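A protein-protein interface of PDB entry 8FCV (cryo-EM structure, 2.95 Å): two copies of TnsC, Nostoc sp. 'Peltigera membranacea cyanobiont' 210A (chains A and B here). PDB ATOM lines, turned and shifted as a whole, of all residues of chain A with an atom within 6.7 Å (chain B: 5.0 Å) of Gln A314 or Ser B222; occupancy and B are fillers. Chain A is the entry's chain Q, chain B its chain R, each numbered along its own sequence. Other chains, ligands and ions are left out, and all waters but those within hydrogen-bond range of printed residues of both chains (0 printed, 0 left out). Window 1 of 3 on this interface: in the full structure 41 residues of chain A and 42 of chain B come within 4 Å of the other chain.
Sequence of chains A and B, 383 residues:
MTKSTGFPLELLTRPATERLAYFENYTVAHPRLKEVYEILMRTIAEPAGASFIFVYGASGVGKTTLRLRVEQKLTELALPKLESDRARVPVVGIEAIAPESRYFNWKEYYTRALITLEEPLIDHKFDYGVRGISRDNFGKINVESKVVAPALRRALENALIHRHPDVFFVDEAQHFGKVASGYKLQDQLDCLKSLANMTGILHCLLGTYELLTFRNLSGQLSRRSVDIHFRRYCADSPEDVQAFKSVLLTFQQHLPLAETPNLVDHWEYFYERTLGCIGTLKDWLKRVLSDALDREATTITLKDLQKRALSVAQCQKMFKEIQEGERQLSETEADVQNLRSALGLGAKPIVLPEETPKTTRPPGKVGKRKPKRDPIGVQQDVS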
ATOM      1  N   LEU A 275     -26.151   9.186  14.726  1.00  0.00           N
ATOM      2  CA  LEU A 275     -25.435   8.713  13.541  1.00  0.00           C
ATOM      3  C   LEU A 275     -26.013   7.416  12.985  1.00  0.00           C
ATOM      4  O   LEU A 275     -25.336   6.700  12.241  1.00  0.00           O
ATOM      5  CB  LEU A 275     -23.939   8.534  13.827  1.00  0.00           C
ATOM      6  CG  LEU A 275     -23.212   9.668  14.548  1.00  0.00           C
ATOM      7  CD1 LEU A 275     -21.725   9.375  14.619  1.00  0.00           C
ATOM      8  CD2 LEU A 275     -23.465  10.998  13.864  1.00  0.00           C
ATOM      9  N   ALA A 309     -28.591  15.067  25.322  1.00  0.00           N
ATOM     10  CA  ALA A 309     -28.022  14.812  24.009  1.00  0.00           C
ATOM     11  C   ALA A 309     -26.498  14.813  24.077  1.00  0.00           C
ATOM     12  O   ALA A 309     -25.886  15.456  24.935  1.00  0.00           O
ATOM     13  CB  ALA A 309     -28.506  15.854  23.002  1.00  0.00           C
ATOM     14  N   LEU A 310     -25.886  14.079  23.156  1.00  0.00           N
ATOM     15  CA  LEU A 310     -24.436  14.011  23.086  1.00  0.00           C
ATOM     16  C   LEU A 310     -23.862  15.319  22.553  1.00  0.00           C
ATOM     17  O   LEU A 310     -24.514  16.047  21.800  1.00  0.00           O
ATOM     18  CB  LEU A 310     -23.992  12.845  22.201  1.00  0.00           C
ATOM     19  CG  LEU A 310     -24.046  11.457  22.842  1.00  0.00           C
ATOM     20  CD1 LEU A 310     -25.371  10.773  22.545  1.00  0.00           C
ATOM     21  CD2 LEU A 310     -22.881  10.602  22.371  1.00  0.00           C
ATOM     22  N   SER A 311     -22.628  15.612  22.956  1.00  0.00           N
ATOM     23  CA  SER A 311     -21.975  16.841  22.533  1.00  0.00           C
ATOM     24  C   SER A 311     -21.672  16.799  21.041  1.00  0.00           C
ATOM     25  O   SER A 311     -21.397  15.738  20.475  1.00  0.00           O
ATOM     26  CB  SER A 311     -20.684  17.056  23.325  1.00  0.00           C
ATOM     27  OG  SER A 311     -20.930  17.017  24.719  1.00  0.00           O
ATOM     28  N   VAL A 312     -21.721  17.971  20.404  1.00  0.00           N
ATOM     29  CA  VAL A 312     -21.504  18.054  18.960  1.00  0.00           C
ATOM     30  C   VAL A 312     -20.108  17.564  18.598  1.00  0.00           C
ATOM     31  O   VAL A 312     -19.921  16.861  17.596  1.00  0.00           O
ATOM     32  CB  VAL A 312     -21.751  19.492  18.466  1.00  0.00           C
ATOM     33  CG1 VAL A 312     -21.158  19.693  17.080  1.00  0.00           C
ATOM     34  CG2 VAL A 312     -23.239  19.798  18.457  1.00  0.00           C
ATOM     35  N   ALA A 313     -19.106  17.924  19.404  1.00  0.00           N
ATOM     36  CA  ALA A 313     -17.746  17.461  19.143  1.00  0.00           C
ATOM     37  C   ALA A 313     -17.654  15.942  19.224  1.00  0.00           C
ATOM     38  O   ALA A 313     -16.964  15.309  18.415  1.00  0.00           O
ATOM     39  CB  ALA A 313     -16.773  18.114  20.122  1.00  0.00           C
ATOM     40  N   GLN A 314     -18.336  15.340  20.202  1.00  0.00           N
ATOM     41  CA  GLN A 314     -18.332  13.886  20.318  1.00  0.00           C
ATOM     42  C   GLN A 314     -18.926  13.231  19.079  1.00  0.00           C
ATOM     43  O   GLN A 314     -18.360  12.267  18.544  1.00  0.00           O
ATOM     44  CB  GLN A 314     -19.099  13.456  21.569  1.00  0.00           C
ATOM     45  CG  GLN A 314     -18.586  14.064  22.863  1.00  0.00           C
ATOM     46  CD  GLN A 314     -19.285  13.500  24.085  1.00  0.00           C
ATOM     47  OE1 GLN A 314     -20.007  14.209  24.784  1.00  0.00           O
ATOM     48  NE2 GLN A 314     -19.073  12.215  24.347  1.00  0.00           N
ATOM     49  N   CYS A 315     -20.069  13.744  18.608  1.00  0.00           N
ATOM     50  CA  CYS A 315     -20.689  13.197  17.407  1.00  0.00           C
ATOM     51  C   CYS A 315     -19.788  13.373  16.195  1.00  0.00           C
ATOM     52  O   CYS A 315     -19.677  12.468  15.360  1.00  0.00           O
ATOM     53  CB  CYS A 315     -22.049  13.853  17.165  1.00  0.00           C
ATOM     54  SG  CYS A 315     -23.116  13.950  18.620  1.00  0.00           S
ATOM     55  N   GLN A 316     -19.128  14.529  16.085  1.00  0.00           N
ATOM     56  CA  GLN A 316     -18.190  14.744  14.989  1.00  0.00           C
ATOM     57  C   GLN A 316     -17.068  13.717  15.024  1.00  0.00           C
ATOM     58  O   GLN A 316     -16.682  13.170  13.984  1.00  0.00           O
ATOM     59  CB  GLN A 316     -17.617  16.158  15.057  1.00  0.00           C
ATOM     60  CG  GLN A 316     -18.458  17.216  14.363  1.00  0.00           C
ATOM     61  CD  GLN A 316     -17.856  18.601  14.484  1.00  0.00           C
ATOM     62  OE1 GLN A 316     -16.921  18.820  15.256  1.00  0.00           O
ATOM     63  NE2 GLN A 316     -18.388  19.548  13.721  1.00  0.00           N
ATOM     64  N   LYS A 317     -16.535  13.439  16.214  1.00  0.00           N
ATOM     65  CA  LYS A 317     -15.432  12.490  16.321  1.00  0.00           C
ATOM     66  C   LYS A 317     -15.870  11.081  15.939  1.00  0.00           C
ATOM     67  O   LYS A 317     -15.182  10.394  15.170  1.00  0.00           O
ATOM     68  CB  LYS A 317     -14.852  12.505  17.734  1.00  0.00           C
ATOM     69  CG  LYS A 317     -13.498  11.832  17.825  1.00  0.00           C
ATOM     70  CD  LYS A 317     -12.431  12.677  17.144  1.00  0.00           C
ATOM     71  CE  LYS A 317     -11.108  11.938  17.057  1.00  0.00           C
ATOM     72  NZ  LYS A 317     -10.909  11.033  18.219  1.00  0.00           N
ATOM     73  N   MET A 318     -17.014  10.624  16.463  1.00  0.00           N
ATOM     74  CA  MET A 318     -17.430   9.268  16.113  1.00  0.00           C
ATOM     75  C   MET A 318     -17.808   9.172  14.642  1.00  0.00           C
ATOM     76  O   MET A 318     -17.563   8.137  14.014  1.00  0.00           O
ATOM     77  CB  MET A 318     -18.592   8.766  16.977  1.00  0.00           C
ATOM     78  CG  MET A 318     -19.575   9.790  17.484  1.00  0.00           C
ATOM     79  SD  MET A 318     -20.535   9.130  18.863  1.00  0.00           S
ATOM     80  CE  MET A 318     -21.993  10.167  18.816  1.00  0.00           C
ATOM     81  N   PHE A 319     -18.388  10.232  14.072  1.00  0.00           N
ATOM     82  CA  PHE A 319     -18.685  10.230  12.646  1.00  0.00           C
ATOM     83  C   PHE A 319     -17.412  10.150  11.817  1.00  0.00           C
ATOM     84  O   PHE A 319     -17.359   9.422  10.822  1.00  0.00           O
ATOM     85  CB  PHE A 319     -19.486  11.472  12.262  1.00  0.00           C
ATOM     86  CG  PHE A 319     -19.755  11.579  10.791  1.00  0.00           C
ATOM     87  CD1 PHE A 319     -20.725  10.795  10.192  1.00  0.00           C
ATOM     88  CD2 PHE A 319     -19.021  12.445  10.001  1.00  0.00           C
ATOM     89  CE1 PHE A 319     -20.970  10.883   8.836  1.00  0.00           C
ATOM     90  CE2 PHE A 319     -19.257  12.536   8.645  1.00  0.00           C
ATOM     91  CZ  PHE A 319     -20.233  11.756   8.062  1.00  0.00           C
ATOM     92  N   ASN B 216     -12.172  13.690  23.441  1.00  0.00           N
ATOM     93  CA  ASN B 216     -12.741  12.821  22.405  1.00  0.00           C
ATOM     94  C   ASN B 216     -11.617  12.154  21.619  1.00  0.00           C
ATOM     95  O   ASN B 216     -11.603  12.153  20.387  1.00  0.00           O
ATOM     96  CB  ASN B 216     -13.668  13.573  21.443  1.00  0.00           C
ATOM     97  CG  ASN B 216     -14.705  14.429  22.147  1.00  0.00           C
ATOM     98  OD1 ASN B 216     -14.847  14.397  23.364  1.00  0.00           O
ATOM     99  ND2 ASN B 216     -15.435  15.214  21.367  1.00  0.00           N
ATOM    100  N   SER B 218     -10.936   9.191  20.948  1.00  0.00           N
ATOM    101  CA  SER B 218     -11.337   8.122  20.040  1.00  0.00           C
ATOM    102  C   SER B 218     -12.848   7.964  20.104  1.00  0.00           C
ATOM    103  O   SER B 218     -13.493   8.372  21.073  1.00  0.00           O
ATOM    104  CB  SER B 218     -10.645   6.797  20.374  1.00  0.00           C
ATOM    105  OG  SER B 218     -10.916   6.403  21.705  1.00  0.00           O
ATOM    106  N   GLY B 219     -13.402   7.349  19.056  1.00  0.00           N
ATOM    107  CA  GLY B 219     -14.848   7.237  18.950  1.00  0.00           C
ATOM    108  C   GLY B 219     -15.460   6.380  20.043  1.00  0.00           C
ATOM    109  O   GLY B 219     -16.520   6.708  20.587  1.00  0.00           O
ATOM    110  N   GLN B 220     -14.808   5.263  20.370  1.00  0.00           N
ATOM    111  CA  GLN B 220     -15.333   4.372  21.402  1.00  0.00           C
ATOM    112  C   GLN B 220     -15.411   5.085  22.746  1.00  0.00           C
ATOM    113  O   GLN B 220     -16.405   4.961  23.472  1.00  0.00           O
ATOM    114  CB  GLN B 220     -14.466   3.118  21.503  1.00  0.00           C
ATOM    115  CG  GLN B 220     -14.995   1.935  20.712  1.00  0.00           C
ATOM    116  CD  GLN B 220     -16.087   1.184  21.446  1.00  0.00           C
ATOM    117  OE1 GLN B 220     -16.334   1.424  22.628  1.00  0.00           O
ATOM    118  NE2 GLN B 220     -16.750   0.271  20.748  1.00  0.00           N
ATOM    119  N   LEU B 221     -14.369   5.840  23.094  1.00  0.00           N
ATOM    120  CA  LEU B 221     -14.409   6.626  24.321  1.00  0.00           C
ATOM    121  C   LEU B 221     -15.305   7.849  24.164  1.00  0.00           C
ATOM    122  O   LEU B 221     -15.876   8.337  25.144  1.00  0.00           O
ATOM    123  CB  LEU B 221     -12.995   7.037  24.729  1.00  0.00           C
ATOM    124  CG  LEU B 221     -12.075   5.886  25.135  1.00  0.00           C
ATOM    125  CD1 LEU B 221     -10.630   6.188  24.794  1.00  0.00           C
ATOM    126  CD2 LEU B 221     -12.221   5.607  26.616  1.00  0.00           C
ATOM    127  N   SER B 222     -15.433   8.361  22.936  1.00  0.00           N
ATOM    128  CA  SER B 222     -16.278   9.526  22.707  1.00  0.00           C
ATOM    129  C   SER B 222     -17.744   9.220  22.990  1.00  0.00           C
ATOM    130  O   SER B 222     -18.430  10.007  23.650  1.00  0.00           O
ATOM    131  CB  SER B 222     -16.105  10.022  21.272  1.00  0.00           C
ATOM    132  OG  SER B 222     -16.888  11.175  21.034  1.00  0.00           O
ATOM    133  N   ARG B 223     -18.241   8.083  22.496  1.00  0.00           N
ATOM    134  CA  ARG B 223     -19.630   7.715  22.759  1.00  0.00           C
ATOM    135  C   ARG B 223     -19.847   7.395  24.234  1.00  0.00           C
ATOM    136  O   ARG B 223     -20.802   7.878  24.852  1.00  0.00           O
ATOM    137  CB  ARG B 223     -20.044   6.524  21.897  1.00  0.00           C
ATOM    138  CG  ARG B 223     -21.009   5.597  22.624  1.00  0.00           C
ATOM    139  CD  ARG B 223     -21.733   4.629  21.723  1.00  0.00           C
ATOM    140  NE  ARG B 223     -22.290   3.533  22.506  1.00  0.00           N
ATOM    141  CZ  ARG B 223     -23.480   2.990  22.296  1.00  0.00           C
ATOM    142  NH1 ARG B 223     -24.289   3.441  21.353  1.00  0.00           N
ATOM    143  NH2 ARG B 223     -23.874   1.975  23.060  1.00  0.00           N
ATOM    144  N   ARG B 224     -18.965   6.586  24.814  1.00  0.00           N
ATOM    145  CA  ARG B 224     -19.173   6.037  26.146  1.00  0.00           C
ATOM    146  C   ARG B 224     -18.858   7.031  27.255  1.00  0.00           C
ATOM    147  O   ARG B 224     -18.761   6.627  28.418  1.00  0.00           O
ATOM    148  CB  ARG B 224     -18.332   4.771  26.319  1.00  0.00           C
ATOM    149  CG  ARG B 224     -18.732   3.651  25.372  1.00  0.00           C
ATOM    150  CD  ARG B 224     -17.963   2.378  25.654  1.00  0.00           C
ATOM    151  NE  ARG B 224     -18.138   1.937  27.032  1.00  0.00           N
ATOM    152  CZ  ARG B 224     -17.601   0.838  27.539  1.00  0.00           C
ATOM    153  NH1 ARG B 224     -16.847   0.034  26.805  1.00  0.00           N
ATOM    154  NH2 ARG B 224     -17.826   0.534  28.813  1.00  0.00           N
ATOM    155  N   SER B 225     -18.696   8.307  26.925  1.00  0.00           N
ATOM    156  CA  SER B 225     -18.415   9.338  27.909  1.00  0.00           C
ATOM    157  C   SER B 225     -19.294  10.550  27.650  1.00  0.00           C
ATOM    158  O   SER B 225     -19.498  10.947  26.499  1.00  0.00           O
ATOM    159  CB  SER B 225     -16.940   9.752  27.873  1.00  0.00           C
ATOM    160  OG  SER B 225     -16.592  10.280  26.606  1.00  0.00           O
ATOM    161  N   VAL B 226     -19.813  11.131  28.727  1.00  0.00           N
ATOM    162  CA  VAL B 226     -20.498  12.415  28.683  1.00  0.00           C
ATOM    163  C   VAL B 226     -19.669  13.405  29.489  1.00  0.00           C
ATOM    164  O   VAL B 226     -18.964  13.019  30.428  1.00  0.00           O
ATOM    165  CB  VAL B 226     -21.941  12.325  29.217  1.00  0.00           C
ATOM    166  CG1 VAL B 226     -22.698  11.211  28.508  1.00  0.00           C
ATOM    167  CG2 VAL B 226     -21.949  12.105  30.717  1.00  0.00           C
ATOM    168  N   ASP B 227     -19.739  14.675  29.110  1.00  0.00           N
ATOM    169  CA  ASP B 227     -18.890  15.704  29.689  1.00  0.00           C
ATOM    170  C   ASP B 227     -19.737  16.758  30.387  1.00  0.00           C
ATOM    171  O   ASP B 227     -20.742  17.225  29.844  1.00  0.00           O
ATOM    172  CB  ASP B 227     -18.011  16.357  28.617  1.00  0.00           C
ATOM    173  CG  ASP B 227     -18.819  16.946  27.477  1.00  0.00           C
ATOM    174  OD1 ASP B 227     -19.692  16.236  26.936  1.00  0.00           O
ATOM    175  OD2 ASP B 227     -18.576  18.119  27.120  1.00  0.00           O
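Of the 12 printed residues of chain A, 4 touch a printed residue of chain B.
Hydrophobic or aromatic side chains of chain A within 4 Å of the printed part of chain B: Ala A313.
Among the printed residues, 8 pairs touch across the chains.
Among the printed residues, no Asp or Glu carboxylate lies within 4 Å of a Lys or Arg side-chain nitrogen of the other chain.
No position is printed for both chains.
Of the 8 pairs that touch across the chains among the printed residues, none has its exchanged pair printed and touching as well.
The side-chain amide oxygen (OE1) of Gln A314 lies within hydrogen-bond range of the side-chain hydroxyl (OG) of Ser A311, at 3.0 Å.
The side-chain sulfur of Cys A315 lies within hydrogen-bond range of the backbone carbonyl oxygen of Ser A311 (3.1 Å).
O of Leu B221 is in hydrogen-bond range of OG of Ser B225 (2.5 Å).
OG of Ser B225 sits at hydrogen-bond distance from O of Ser B222 (3.5 Å).
Of the printed residues of chain B, Ala A313 touches Asn B216.
Printed residues of chain A within 4 Å of Asn B216: Ala A313, Gln A314 and Lys A317.
Of the printed residues of chain A, Ser B222 touches Gln A314.
Printed residues of chain A within 4 Å of Ser B225: Gln A314.
The nearest residue of chain A that does not touch Ser B222 is Lys A317 (4.1 Å).
The nearest printed residue of chain B that does not touch Ala A313 is Ser B222 (4.9 Å).
The side-chain hydroxyl (OG) of Ser A311 lies within hydrogen-bond range of the side-chain carboxylate (OD1) of Asp B227 (2.7 Å).
The side-chain amide nitrogen (ND2) of Asn B216 lies close to the backbone carbonyl oxygen (O) of Ala A313 (3.3 Å).
N of Gln A314 lies close to ND2 of Asn B216 (3.1 Å).
NE2 of Gln A314 is in hydrogen-bond range of O of Ser B222, 2.4 Å away.
The backbone carbonyl oxygen (O) of Ser B225 lies within hydrogen-bond range of the side-chain amide nitrogen (NE2) of Gln A314 (2.5 Å).
The side-chain amide oxygen (OE1) of Gln A314 lies close to the side-chain carboxylate (OD1) of Asp B227 (3.0 Å).
NZ of Lys A317 lies within hydrogen-bond range of O of Asn B216, 2.5 Å away.
The backbone NH (N) of Ser B218 sits close to the side-chain amino group (NZ) of Lys A317 (3.3 Å).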
